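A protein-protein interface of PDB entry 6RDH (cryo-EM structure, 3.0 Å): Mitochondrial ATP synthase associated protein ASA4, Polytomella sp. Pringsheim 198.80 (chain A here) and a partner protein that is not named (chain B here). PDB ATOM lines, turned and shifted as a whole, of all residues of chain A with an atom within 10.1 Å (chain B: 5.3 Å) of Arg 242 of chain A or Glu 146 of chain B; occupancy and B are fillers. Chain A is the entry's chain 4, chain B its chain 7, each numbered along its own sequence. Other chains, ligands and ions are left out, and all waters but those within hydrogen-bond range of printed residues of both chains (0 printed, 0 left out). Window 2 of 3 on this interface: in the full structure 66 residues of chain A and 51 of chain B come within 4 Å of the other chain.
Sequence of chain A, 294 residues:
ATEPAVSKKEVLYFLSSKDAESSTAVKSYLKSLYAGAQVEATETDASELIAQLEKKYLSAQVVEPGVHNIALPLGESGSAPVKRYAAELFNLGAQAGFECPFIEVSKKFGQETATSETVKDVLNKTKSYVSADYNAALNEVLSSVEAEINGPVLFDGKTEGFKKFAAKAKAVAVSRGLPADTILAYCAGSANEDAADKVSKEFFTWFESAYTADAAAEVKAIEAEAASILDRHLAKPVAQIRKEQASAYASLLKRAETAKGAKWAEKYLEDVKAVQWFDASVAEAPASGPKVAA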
ATOM      1  N   LEU A 230      23.985  15.671  -6.590  1.00  0.00           N
ATOM      2  CA  LEU A 230      24.497  15.068  -7.812  1.00  0.00           C
ATOM      3  C   LEU A 230      25.544  14.012  -7.516  1.00  0.00           C
ATOM      4  O   LEU A 230      25.509  12.927  -8.102  1.00  0.00           O
ATOM      5  CB  LEU A 230      25.085  16.136  -8.720  1.00  0.00           C
ATOM      6  CG  LEU A 230      25.578  15.614 -10.057  1.00  0.00           C
ATOM      7  CD1 LEU A 230      24.427  15.341 -10.970  1.00  0.00           C
ATOM      8  CD2 LEU A 230      26.497  16.594 -10.673  1.00  0.00           C
ATOM      9  N   HIS A 233      23.989  11.026  -6.486  1.00  0.00           N
ATOM     10  CA  HIS A 233      23.252  10.414  -7.583  1.00  0.00           C
ATOM     11  C   HIS A 233      24.180   9.806  -8.621  1.00  0.00           C
ATOM     12  O   HIS A 233      23.829   8.802  -9.241  1.00  0.00           O
ATOM     13  CB  HIS A 233      22.323  11.469  -8.190  1.00  0.00           C
ATOM     14  CG  HIS A 233      21.949  11.245  -9.620  1.00  0.00           C
ATOM     15  ND1 HIS A 233      22.724  11.682 -10.669  1.00  0.00           N
ATOM     16  CD2 HIS A 233      20.837  10.716 -10.173  1.00  0.00           C
ATOM     17  CE1 HIS A 233      22.131  11.384 -11.808  1.00  0.00           C
ATOM     18  NE2 HIS A 233      20.983  10.798 -11.535  1.00  0.00           N
ATOM     19  N   LEU A 234      25.375  10.366  -8.802  1.00  0.00           N
ATOM     20  CA  LEU A 234      26.315   9.829  -9.778  1.00  0.00           C
ATOM     21  C   LEU A 234      26.992   8.549  -9.320  1.00  0.00           C
ATOM     22  O   LEU A 234      27.738   7.957 -10.102  1.00  0.00           O
ATOM     23  CB  LEU A 234      27.385  10.862 -10.105  1.00  0.00           C
ATOM     24  CG  LEU A 234      26.973  12.039 -10.970  1.00  0.00           C
ATOM     25  CD1 LEU A 234      28.190  12.794 -11.371  1.00  0.00           C
ATOM     26  CD2 LEU A 234      26.227  11.583 -12.186  1.00  0.00           C
ATOM     27  N   LYS A 236      25.220   5.915  -8.218  1.00  0.00           N
ATOM     28  CA  LYS A 236      24.267   4.845  -8.447  1.00  0.00           C
ATOM     29  C   LYS A 236      24.399   4.306  -9.865  1.00  0.00           C
ATOM     30  O   LYS A 236      24.864   5.011 -10.760  1.00  0.00           O
ATOM     31  CB  LYS A 236      22.849   5.351  -8.237  1.00  0.00           C
ATOM     32  CG  LYS A 236      22.641   6.104  -6.953  1.00  0.00           C
ATOM     33  CD  LYS A 236      21.199   6.537  -6.822  1.00  0.00           C
ATOM     34  CE  LYS A 236      21.020   7.498  -5.675  1.00  0.00           C
ATOM     35  NZ  LYS A 236      21.520   6.926  -4.407  1.00  0.00           N
ATOM     36  N   PRO A 237      24.017   3.057 -10.114  1.00  0.00           N
ATOM     37  CA  PRO A 237      23.867   2.601 -11.494  1.00  0.00           C
ATOM     38  C   PRO A 237      22.634   3.223 -12.119  1.00  0.00           C
ATOM     39  O   PRO A 237      21.789   3.804 -11.444  1.00  0.00           O
ATOM     40  CB  PRO A 237      23.725   1.089 -11.356  1.00  0.00           C
ATOM     41  CG  PRO A 237      23.234   0.892  -9.989  1.00  0.00           C
ATOM     42  CD  PRO A 237      23.881   1.944  -9.166  1.00  0.00           C
ATOM     43  N   VAL A 238      22.529   3.076 -13.437  1.00  0.00           N
ATOM     44  CA  VAL A 238      21.521   3.821 -14.179  1.00  0.00           C
ATOM     45  C   VAL A 238      20.133   3.256 -13.942  1.00  0.00           C
ATOM     46  O   VAL A 238      19.150   4.002 -13.929  1.00  0.00           O
ATOM     47  CB  VAL A 238      21.877   3.826 -15.668  1.00  0.00           C
ATOM     48  CG1 VAL A 238      21.131   4.913 -16.375  1.00  0.00           C
ATOM     49  CG2 VAL A 238      23.348   4.006 -15.838  1.00  0.00           C
ATOM     50  N   ALA A 239      20.023   1.944 -13.729  1.00  0.00           N
ATOM     51  CA  ALA A 239      18.716   1.332 -13.525  1.00  0.00           C
ATOM     52  C   ALA A 239      18.103   1.736 -12.195  1.00  0.00           C
ATOM     53  O   ALA A 239      16.884   1.924 -12.108  1.00  0.00           O
ATOM     54  CB  ALA A 239      18.831  -0.184 -13.610  1.00  0.00           C
ATOM     55  N   GLN A 240      18.935   1.895 -11.164  1.00  0.00           N
ATOM     56  CA  GLN A 240      18.450   2.371  -9.874  1.00  0.00           C
ATOM     57  C   GLN A 240      17.956   3.802  -9.974  1.00  0.00           C
ATOM     58  O   GLN A 240      16.919   4.144  -9.398  1.00  0.00           O
ATOM     59  CB  GLN A 240      19.555   2.263  -8.830  1.00  0.00           C
ATOM     60  CG  GLN A 240      19.149   2.735  -7.459  1.00  0.00           C
ATOM     61  CD  GLN A 240      20.320   2.848  -6.514  1.00  0.00           C
ATOM     62  OE1 GLN A 240      20.219   3.458  -5.452  1.00  0.00           O
ATOM     63  NE2 GLN A 240      21.441   2.252  -6.890  1.00  0.00           N
ATOM     64  N   ILE A 241      18.676   4.638 -10.725  1.00  0.00           N
ATOM     65  CA  ILE A 241      18.283   6.030 -10.934  1.00  0.00           C
ATOM     66  C   ILE A 241      16.962   6.105 -11.674  1.00  0.00           C
ATOM     67  O   ILE A 241      16.060   6.859 -11.287  1.00  0.00           O
ATOM     68  CB  ILE A 241      19.393   6.773 -11.691  1.00  0.00           C
ATOM     69  CG1 ILE A 241      20.587   6.984 -10.786  1.00  0.00           C
ATOM     70  CG2 ILE A 241      18.912   8.090 -12.220  1.00  0.00           C
ATOM     71  CD1 ILE A 241      21.761   7.449 -11.521  1.00  0.00           C
ATOM     72  N   ARG A 242      16.810   5.292 -12.718  1.00  0.00           N
ATOM     73  CA  ARG A 242      15.590   5.324 -13.509  1.00  0.00           C
ATOM     74  C   ARG A 242      14.390   4.824 -12.715  1.00  0.00           C
ATOM     75  O   ARG A 242      13.319   5.437 -12.767  1.00  0.00           O
ATOM     76  CB  ARG A 242      15.772   4.510 -14.781  1.00  0.00           C
ATOM     77  CG  ARG A 242      16.708   5.144 -15.773  1.00  0.00           C
ATOM     78  CD  ARG A 242      16.464   4.611 -17.155  1.00  0.00           C
ATOM     79  NE  ARG A 242      17.480   5.064 -18.093  1.00  0.00           N
ATOM     80  CZ  ARG A 242      18.421   4.280 -18.600  1.00  0.00           C
ATOM     81  NH1 ARG A 242      18.470   3.001 -18.262  1.00  0.00           N
ATOM     82  NH2 ARG A 242      19.310   4.775 -19.444  1.00  0.00           N
ATOM     83  N   LYS A 243      14.555   3.755 -11.931  1.00  0.00           N
ATOM     84  CA  LYS A 243      13.408   3.272 -11.171  1.00  0.00           C
ATOM     85  C   LYS A 243      13.095   4.156  -9.970  1.00  0.00           C
ATOM     86  O   LYS A 243      11.918   4.318  -9.634  1.00  0.00           O
ATOM     87  CB  LYS A 243      13.606   1.815 -10.739  1.00  0.00           C
ATOM     88  CG  LYS A 243      14.645   1.553  -9.669  1.00  0.00           C
ATOM     89  CD  LYS A 243      14.268   0.335  -8.842  1.00  0.00           C
ATOM     90  CE  LYS A 243      15.412  -0.112  -7.948  1.00  0.00           C
ATOM     91  NZ  LYS A 243      16.497  -0.773  -8.721  1.00  0.00           N
ATOM     92  N   GLU A 244      14.107   4.788  -9.356  1.00  0.00           N
ATOM     93  CA  GLU A 244      13.852   5.710  -8.255  1.00  0.00           C
ATOM     94  C   GLU A 244      13.120   6.951  -8.738  1.00  0.00           C
ATOM     95  O   GLU A 244      12.141   7.381  -8.119  1.00  0.00           O
ATOM     96  CB  GLU A 244      15.165   6.104  -7.585  1.00  0.00           C
ATOM     97  CG  GLU A 244      15.650   5.158  -6.505  1.00  0.00           C
ATOM     98  CD  GLU A 244      16.923   5.651  -5.830  1.00  0.00           C
ATOM     99  OE1 GLU A 244      17.561   6.583  -6.364  1.00  0.00           O
ATOM    100  OE2 GLU A 244      17.282   5.109  -4.763  1.00  0.00           O
ATOM    101  N   GLN A 245      13.557   7.515  -9.864  1.00  0.00           N
ATOM    102  CA  GLN A 245      12.900   8.701 -10.390  1.00  0.00           C
ATOM    103  C   GLN A 245      11.522   8.390 -10.945  1.00  0.00           C
ATOM    104  O   GLN A 245      10.612   9.215 -10.818  1.00  0.00           O
ATOM    105  CB  GLN A 245      13.768   9.339 -11.460  1.00  0.00           C
ATOM    106  CG  GLN A 245      15.013   9.974 -10.918  1.00  0.00           C
ATOM    107  CD  GLN A 245      15.612  10.931 -11.894  1.00  0.00           C
ATOM    108  OE1 GLN A 245      15.260  10.925 -13.067  1.00  0.00           O
ATOM    109  NE2 GLN A 245      16.510  11.776 -11.421  1.00  0.00           N
ATOM    110  N   ALA A 246      11.333   7.206 -11.535  1.00  0.00           N
ATOM    111  CA  ALA A 246      10.010   6.836 -12.015  1.00  0.00           C
ATOM    112  C   ALA A 246       9.051   6.598 -10.860  1.00  0.00           C
ATOM    113  O   ALA A 246       7.874   6.963 -10.945  1.00  0.00           O
ATOM    114  CB  ALA A 246      10.103   5.598 -12.898  1.00  0.00           C
ATOM    115  N   SER A 247       9.544   6.029  -9.756  1.00  0.00           N
ATOM    116  CA  SER A 247       8.702   5.826  -8.584  1.00  0.00           C
ATOM    117  C   SER A 247       8.339   7.147  -7.925  1.00  0.00           C
ATOM    118  O   SER A 247       7.198   7.329  -7.485  1.00  0.00           O
ATOM    119  CB  SER A 247       9.409   4.915  -7.590  1.00  0.00           C
ATOM    120  OG  SER A 247       9.682   3.657  -8.176  1.00  0.00           O
ATOM    121  N   ALA A 248       9.286   8.091  -7.873  1.00  0.00           N
ATOM    122  CA  ALA A 248       8.994   9.402  -7.300  1.00  0.00           C
ATOM    123  C   ALA A 248       8.003  10.181  -8.156  1.00  0.00           C
ATOM    124  O   ALA A 248       7.077  10.805  -7.623  1.00  0.00           O
ATOM    125  CB  ALA A 248      10.283  10.197  -7.122  1.00  0.00           C
ATOM    126  N   TYR A 249       8.168  10.130  -9.483  1.00  0.00           N
ATOM    127  CA  TYR A 249       7.225  10.773 -10.389  1.00  0.00           C
ATOM    128  C   TYR A 249       5.841  10.161 -10.273  1.00  0.00           C
ATOM    129  O   TYR A 249       4.842  10.886 -10.232  1.00  0.00           O
ATOM    130  CB  TYR A 249       7.726  10.663 -11.826  1.00  0.00           C
ATOM    131  CG  TYR A 249       6.846  11.327 -12.858  1.00  0.00           C
ATOM    132  CD1 TYR A 249       6.993  12.665 -13.153  1.00  0.00           C
ATOM    133  CD2 TYR A 249       5.887  10.607 -13.556  1.00  0.00           C
ATOM    134  CE1 TYR A 249       6.204  13.269 -14.095  1.00  0.00           C
ATOM    135  CE2 TYR A 249       5.088  11.208 -14.488  1.00  0.00           C
ATOM    136  CZ  TYR A 249       5.252  12.537 -14.755  1.00  0.00           C
ATOM    137  OH  TYR A 249       4.459  13.134 -15.698  1.00  0.00           O
ATOM    138  N   ALA A 250       5.761   8.832 -10.221  1.00  0.00           N
ATOM    139  CA  ALA A 250       4.464   8.172 -10.182  1.00  0.00           C
ATOM    140  C   ALA A 250       3.760   8.406  -8.855  1.00  0.00           C
ATOM    141  O   ALA A 250       2.537   8.571  -8.823  1.00  0.00           O
ATOM    142  CB  ALA A 250       4.638   6.683 -10.446  1.00  0.00           C
ATOM    143  N   GLU B 142      28.047   5.376 -17.957  1.00  0.00           N
ATOM    144  CA  GLU B 142      26.634   5.253 -18.269  1.00  0.00           C
ATOM    145  C   GLU B 142      25.786   6.109 -17.346  1.00  0.00           C
ATOM    146  O   GLU B 142      24.707   6.548 -17.741  1.00  0.00           O
ATOM    147  CB  GLU B 142      26.200   3.792 -18.190  1.00  0.00           C
ATOM    148  CG  GLU B 142      26.453   2.986 -19.456  1.00  0.00           C
ATOM    149  CD  GLU B 142      26.313   1.490 -19.239  1.00  0.00           C
ATOM    150  OE1 GLU B 142      26.215   1.055 -18.073  1.00  0.00           O
ATOM    151  OE2 GLU B 142      26.302   0.745 -20.238  1.00  0.00           O
ATOM    152  N   THR B 143      26.247   6.361 -16.121  1.00  0.00           N
ATOM    153  CA  THR B 143      25.448   7.192 -15.230  1.00  0.00           C
ATOM    154  C   THR B 143      25.797   8.673 -15.276  1.00  0.00           C
ATOM    155  O   THR B 143      24.970   9.483 -14.864  1.00  0.00           O
ATOM    156  CB  THR B 143      25.539   6.713 -13.781  1.00  0.00           C
ATOM    157  OG1 THR B 143      24.648   7.492 -12.991  1.00  0.00           O
ATOM    158  CG2 THR B 143      26.911   6.890 -13.216  1.00  0.00           C
ATOM    159  N   VAL B 144      26.972   9.068 -15.768  1.00  0.00           N
ATOM    160  CA  VAL B 144      27.236  10.502 -15.844  1.00  0.00           C
ATOM    161  C   VAL B 144      26.602  11.105 -17.088  1.00  0.00           C
ATOM    162  O   VAL B 144      26.405  12.321 -17.151  1.00  0.00           O
ATOM    163  CB  VAL B 144      28.744  10.807 -15.793  1.00  0.00           C
ATOM    164  CG1 VAL B 144      29.394  10.605 -17.126  1.00  0.00           C
ATOM    165  CG2 VAL B 144      29.009  12.193 -15.274  1.00  0.00           C
ATOM    166  N   THR B 145      26.231  10.283 -18.064  1.00  0.00           N
ATOM    167  CA  THR B 145      25.596  10.750 -19.283  1.00  0.00           C
ATOM    168  C   THR B 145      24.096  10.527 -19.271  1.00  0.00           C
ATOM    169  O   THR B 145      23.451  10.665 -20.307  1.00  0.00           O
ATOM    170  CB  THR B 145      26.221  10.071 -20.487  1.00  0.00           C
ATOM    171  OG1 THR B 145      25.975   8.671 -20.410  1.00  0.00           O
ATOM    172  CG2 THR B 145      27.684  10.278 -20.455  1.00  0.00           C
ATOM    173  N   GLU B 146      23.524  10.184 -18.123  1.00  0.00           N
ATOM    174  CA  GLU B 146      22.077  10.178 -17.958  1.00  0.00           C
ATOM    175  C   GLU B 146      21.651  11.607 -17.638  1.00  0.00           C
ATOM    176  O   GLU B 146      21.446  11.993 -16.488  1.00  0.00           O
ATOM    177  CB  GLU B 146      21.670   9.197 -16.869  1.00  0.00           C
ATOM    178  CG  GLU B 146      20.184   8.977 -16.731  1.00  0.00           C
ATOM    179  CD  GLU B 146      19.593   8.272 -17.917  1.00  0.00           C
ATOM    180  OE1 GLU B 146      20.264   7.374 -18.456  1.00  0.00           O
ATOM    181  OE2 GLU B 146      18.462   8.613 -18.321  1.00  0.00           O
ATOM    182  N   PHE B 147      21.547  12.421 -18.689  1.00  0.00           N
ATOM    183  CA  PHE B 147      21.161  13.813 -18.532  1.00  0.00           C
ATOM    184  C   PHE B 147      19.657  14.002 -18.439  1.00  0.00           C
ATOM    185  O   PHE B 147      19.212  15.116 -18.161  1.00  0.00           O
ATOM    186  CB  PHE B 147      21.693  14.658 -19.686  1.00  0.00           C
ATOM    187  CG  PHE B 147      23.173  14.598 -19.855  1.00  0.00           C
ATOM    188  CD1 PHE B 147      24.012  15.051 -18.873  1.00  0.00           C
ATOM    189  CD2 PHE B 147      23.724  14.096 -21.008  1.00  0.00           C
ATOM    190  CE1 PHE B 147      25.373  14.992 -19.039  1.00  0.00           C
ATOM    191  CE2 PHE B 147      25.072  14.042 -21.180  1.00  0.00           C
ATOM    192  CZ  PHE B 147      25.897  14.493 -20.196  1.00  0.00           C
ATOM    193  N   ASP B 148      18.864  12.964 -18.665  1.00  0.00           N
ATOM    194  CA  ASP B 148      17.434  13.030 -18.398  1.00  0.00           C
ATOM    195  C   ASP B 148      17.095  12.784 -16.937  1.00  0.00           C
ATOM    196  O   ASP B 148      15.920  12.629 -16.605  1.00  0.00           O
ATOM    197  CB  ASP B 148      16.672  12.024 -19.257  1.00  0.00           C
ATOM    198  CG  ASP B 148      16.604  12.426 -20.708  1.00  0.00           C
ATOM    199  OD1 ASP B 148      16.682  13.631 -21.002  1.00  0.00           O
ATOM    200  OD2 ASP B 148      16.440  11.532 -21.561  1.00  0.00           O
ATOM    201  N   SER B 149      18.096  12.718 -16.068  1.00  0.00           N
ATOM    202  CA  SER B 149      17.891  12.631 -14.635  1.00  0.00           C
ATOM    203  C   SER B 149      18.108  13.957 -13.930  1.00  0.00           C
ATOM    204  O   SER B 149      17.717  14.102 -12.764  1.00  0.00           O
ATOM    205  CB  SER B 149      18.840  11.593 -14.043  1.00  0.00           C
ATOM    206  OG  SER B 149      18.796  11.625 -12.634  1.00  0.00           O
ATOM    207  N   LEU B 150      18.707  14.929 -14.618  1.00  0.00           N
ATOM    208  CA  LEU B 150      19.063  16.185 -13.981  1.00  0.00           C
ATOM    209  C   LEU B 150      17.843  17.036 -13.686  1.00  0.00           C
ATOM    210  O   LEU B 150      17.877  17.852 -12.764  1.00  0.00           O
ATOM    211  CB  LEU B 150      20.039  16.950 -14.859  1.00  0.00           C
ATOM    212  CG  LEU B 150      21.327  16.204 -15.146  1.00  0.00           C
ATOM    213  CD1 LEU B 150      22.242  17.096 -15.919  1.00  0.00           C
ATOM    214  CD2 LEU B 150      21.976  15.758 -13.866  1.00  0.00           C
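A ring nitrogen (NE2) of His 233 of chain A lies within hydrogen-bond range of the side-chain hydroxyl (OG) of Ser 149 of chain B, 2.6 Å away. The backbone carbonyl oxygen (O) of Lys 236 of chain A lies within hydrogen-bond range of the side-chain hydroxyl (OG1) of Thr 143 of chain B. The side-chain carboxylate (OE1) of Glu 146 of chain B is in salt-bridge range of the guanidinium group (NH2) of Arg 242 of chain A, at 2.9 Å. NE2 of Gln 245 of chain A is in hydrogen-bond range of OG of Ser 149 of chain B, at 2.6 Å.
Of the printed residues of chain B, Val 238 of chain A touches Glu 142 (3.5 Å), Thr 143 (3.7 Å) and Glu 146 (3.3 Å). Of the printed residues of chain B, Ile 241 of chain A touches Thr 143 (3.2 Å) and Ser 149 (3.6 Å). Of chain B, only Glu 146 comes within 4 Å of Arg 242 of chain A. Of the printed residues of chain A, Glu 142 of chain B touches Val 238 (3.5 Å). No residue of chain A comes within 4 Å of Thr 145 of chain B. Of chain A, only Val 238 (3.3 Å) and Arg 242 (2.9 Å) come within 4 Å of Glu 146 of chain B. No residue of chain A comes within 4 Å of Phe 147 of chain B. Of the printed residues of chain A, Asp 148 of chain B touches Gln 245 (3.98 Å). Ser 149 of chain B touches just these residues of chain A: His 233, Ile 241 and Gln 245. The nearest printed residue of chain B that does not touch Arg 242 of chain A is Glu 142 of chain B (5.9 Å). The nearest printed residue of chain A that does not touch Glu 146 of chain B is His 233 of chain A (4.8 Å).
Hydrophobic or aromatic side chains of chain A that line the printed part of chain B: Leu 230, His 233, Leu 234, Val 238 and Ile 241. Printed residues of chain B that touch a printed residue of chain A: Glu 142, Thr 143, Val 144, Glu 146, Asp 148, Ser 149 and Leu 150. Among the printed residues, 13 pairs touch across the chains. Among the printed residues, Asp or Glu carboxylates within 4 Å of a Lys or Arg side-chain nitrogen of the other chain: Arg 242 of chain A with Glu 146 of chain B.
Among the printed residues, pairs that only touch across the chains: Leu 230 of chain A with Leu 150 of chain B, Leu 234 of chain A with Thr 143 of chain B, Leu 234 of chain A with Val 144 of chain B, Val 238 of chain A with Glu 142 of chain B, Val 238 of chain A with Thr 143 of chain B, Val 238 of chain A with Glu 146 of chain B, Ile 241 of chain A with Thr 143 of chain B, Ile 241 of chain A with Ser 149 of chain B and Gln 245 of chain A with Asp 148 of chain B.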
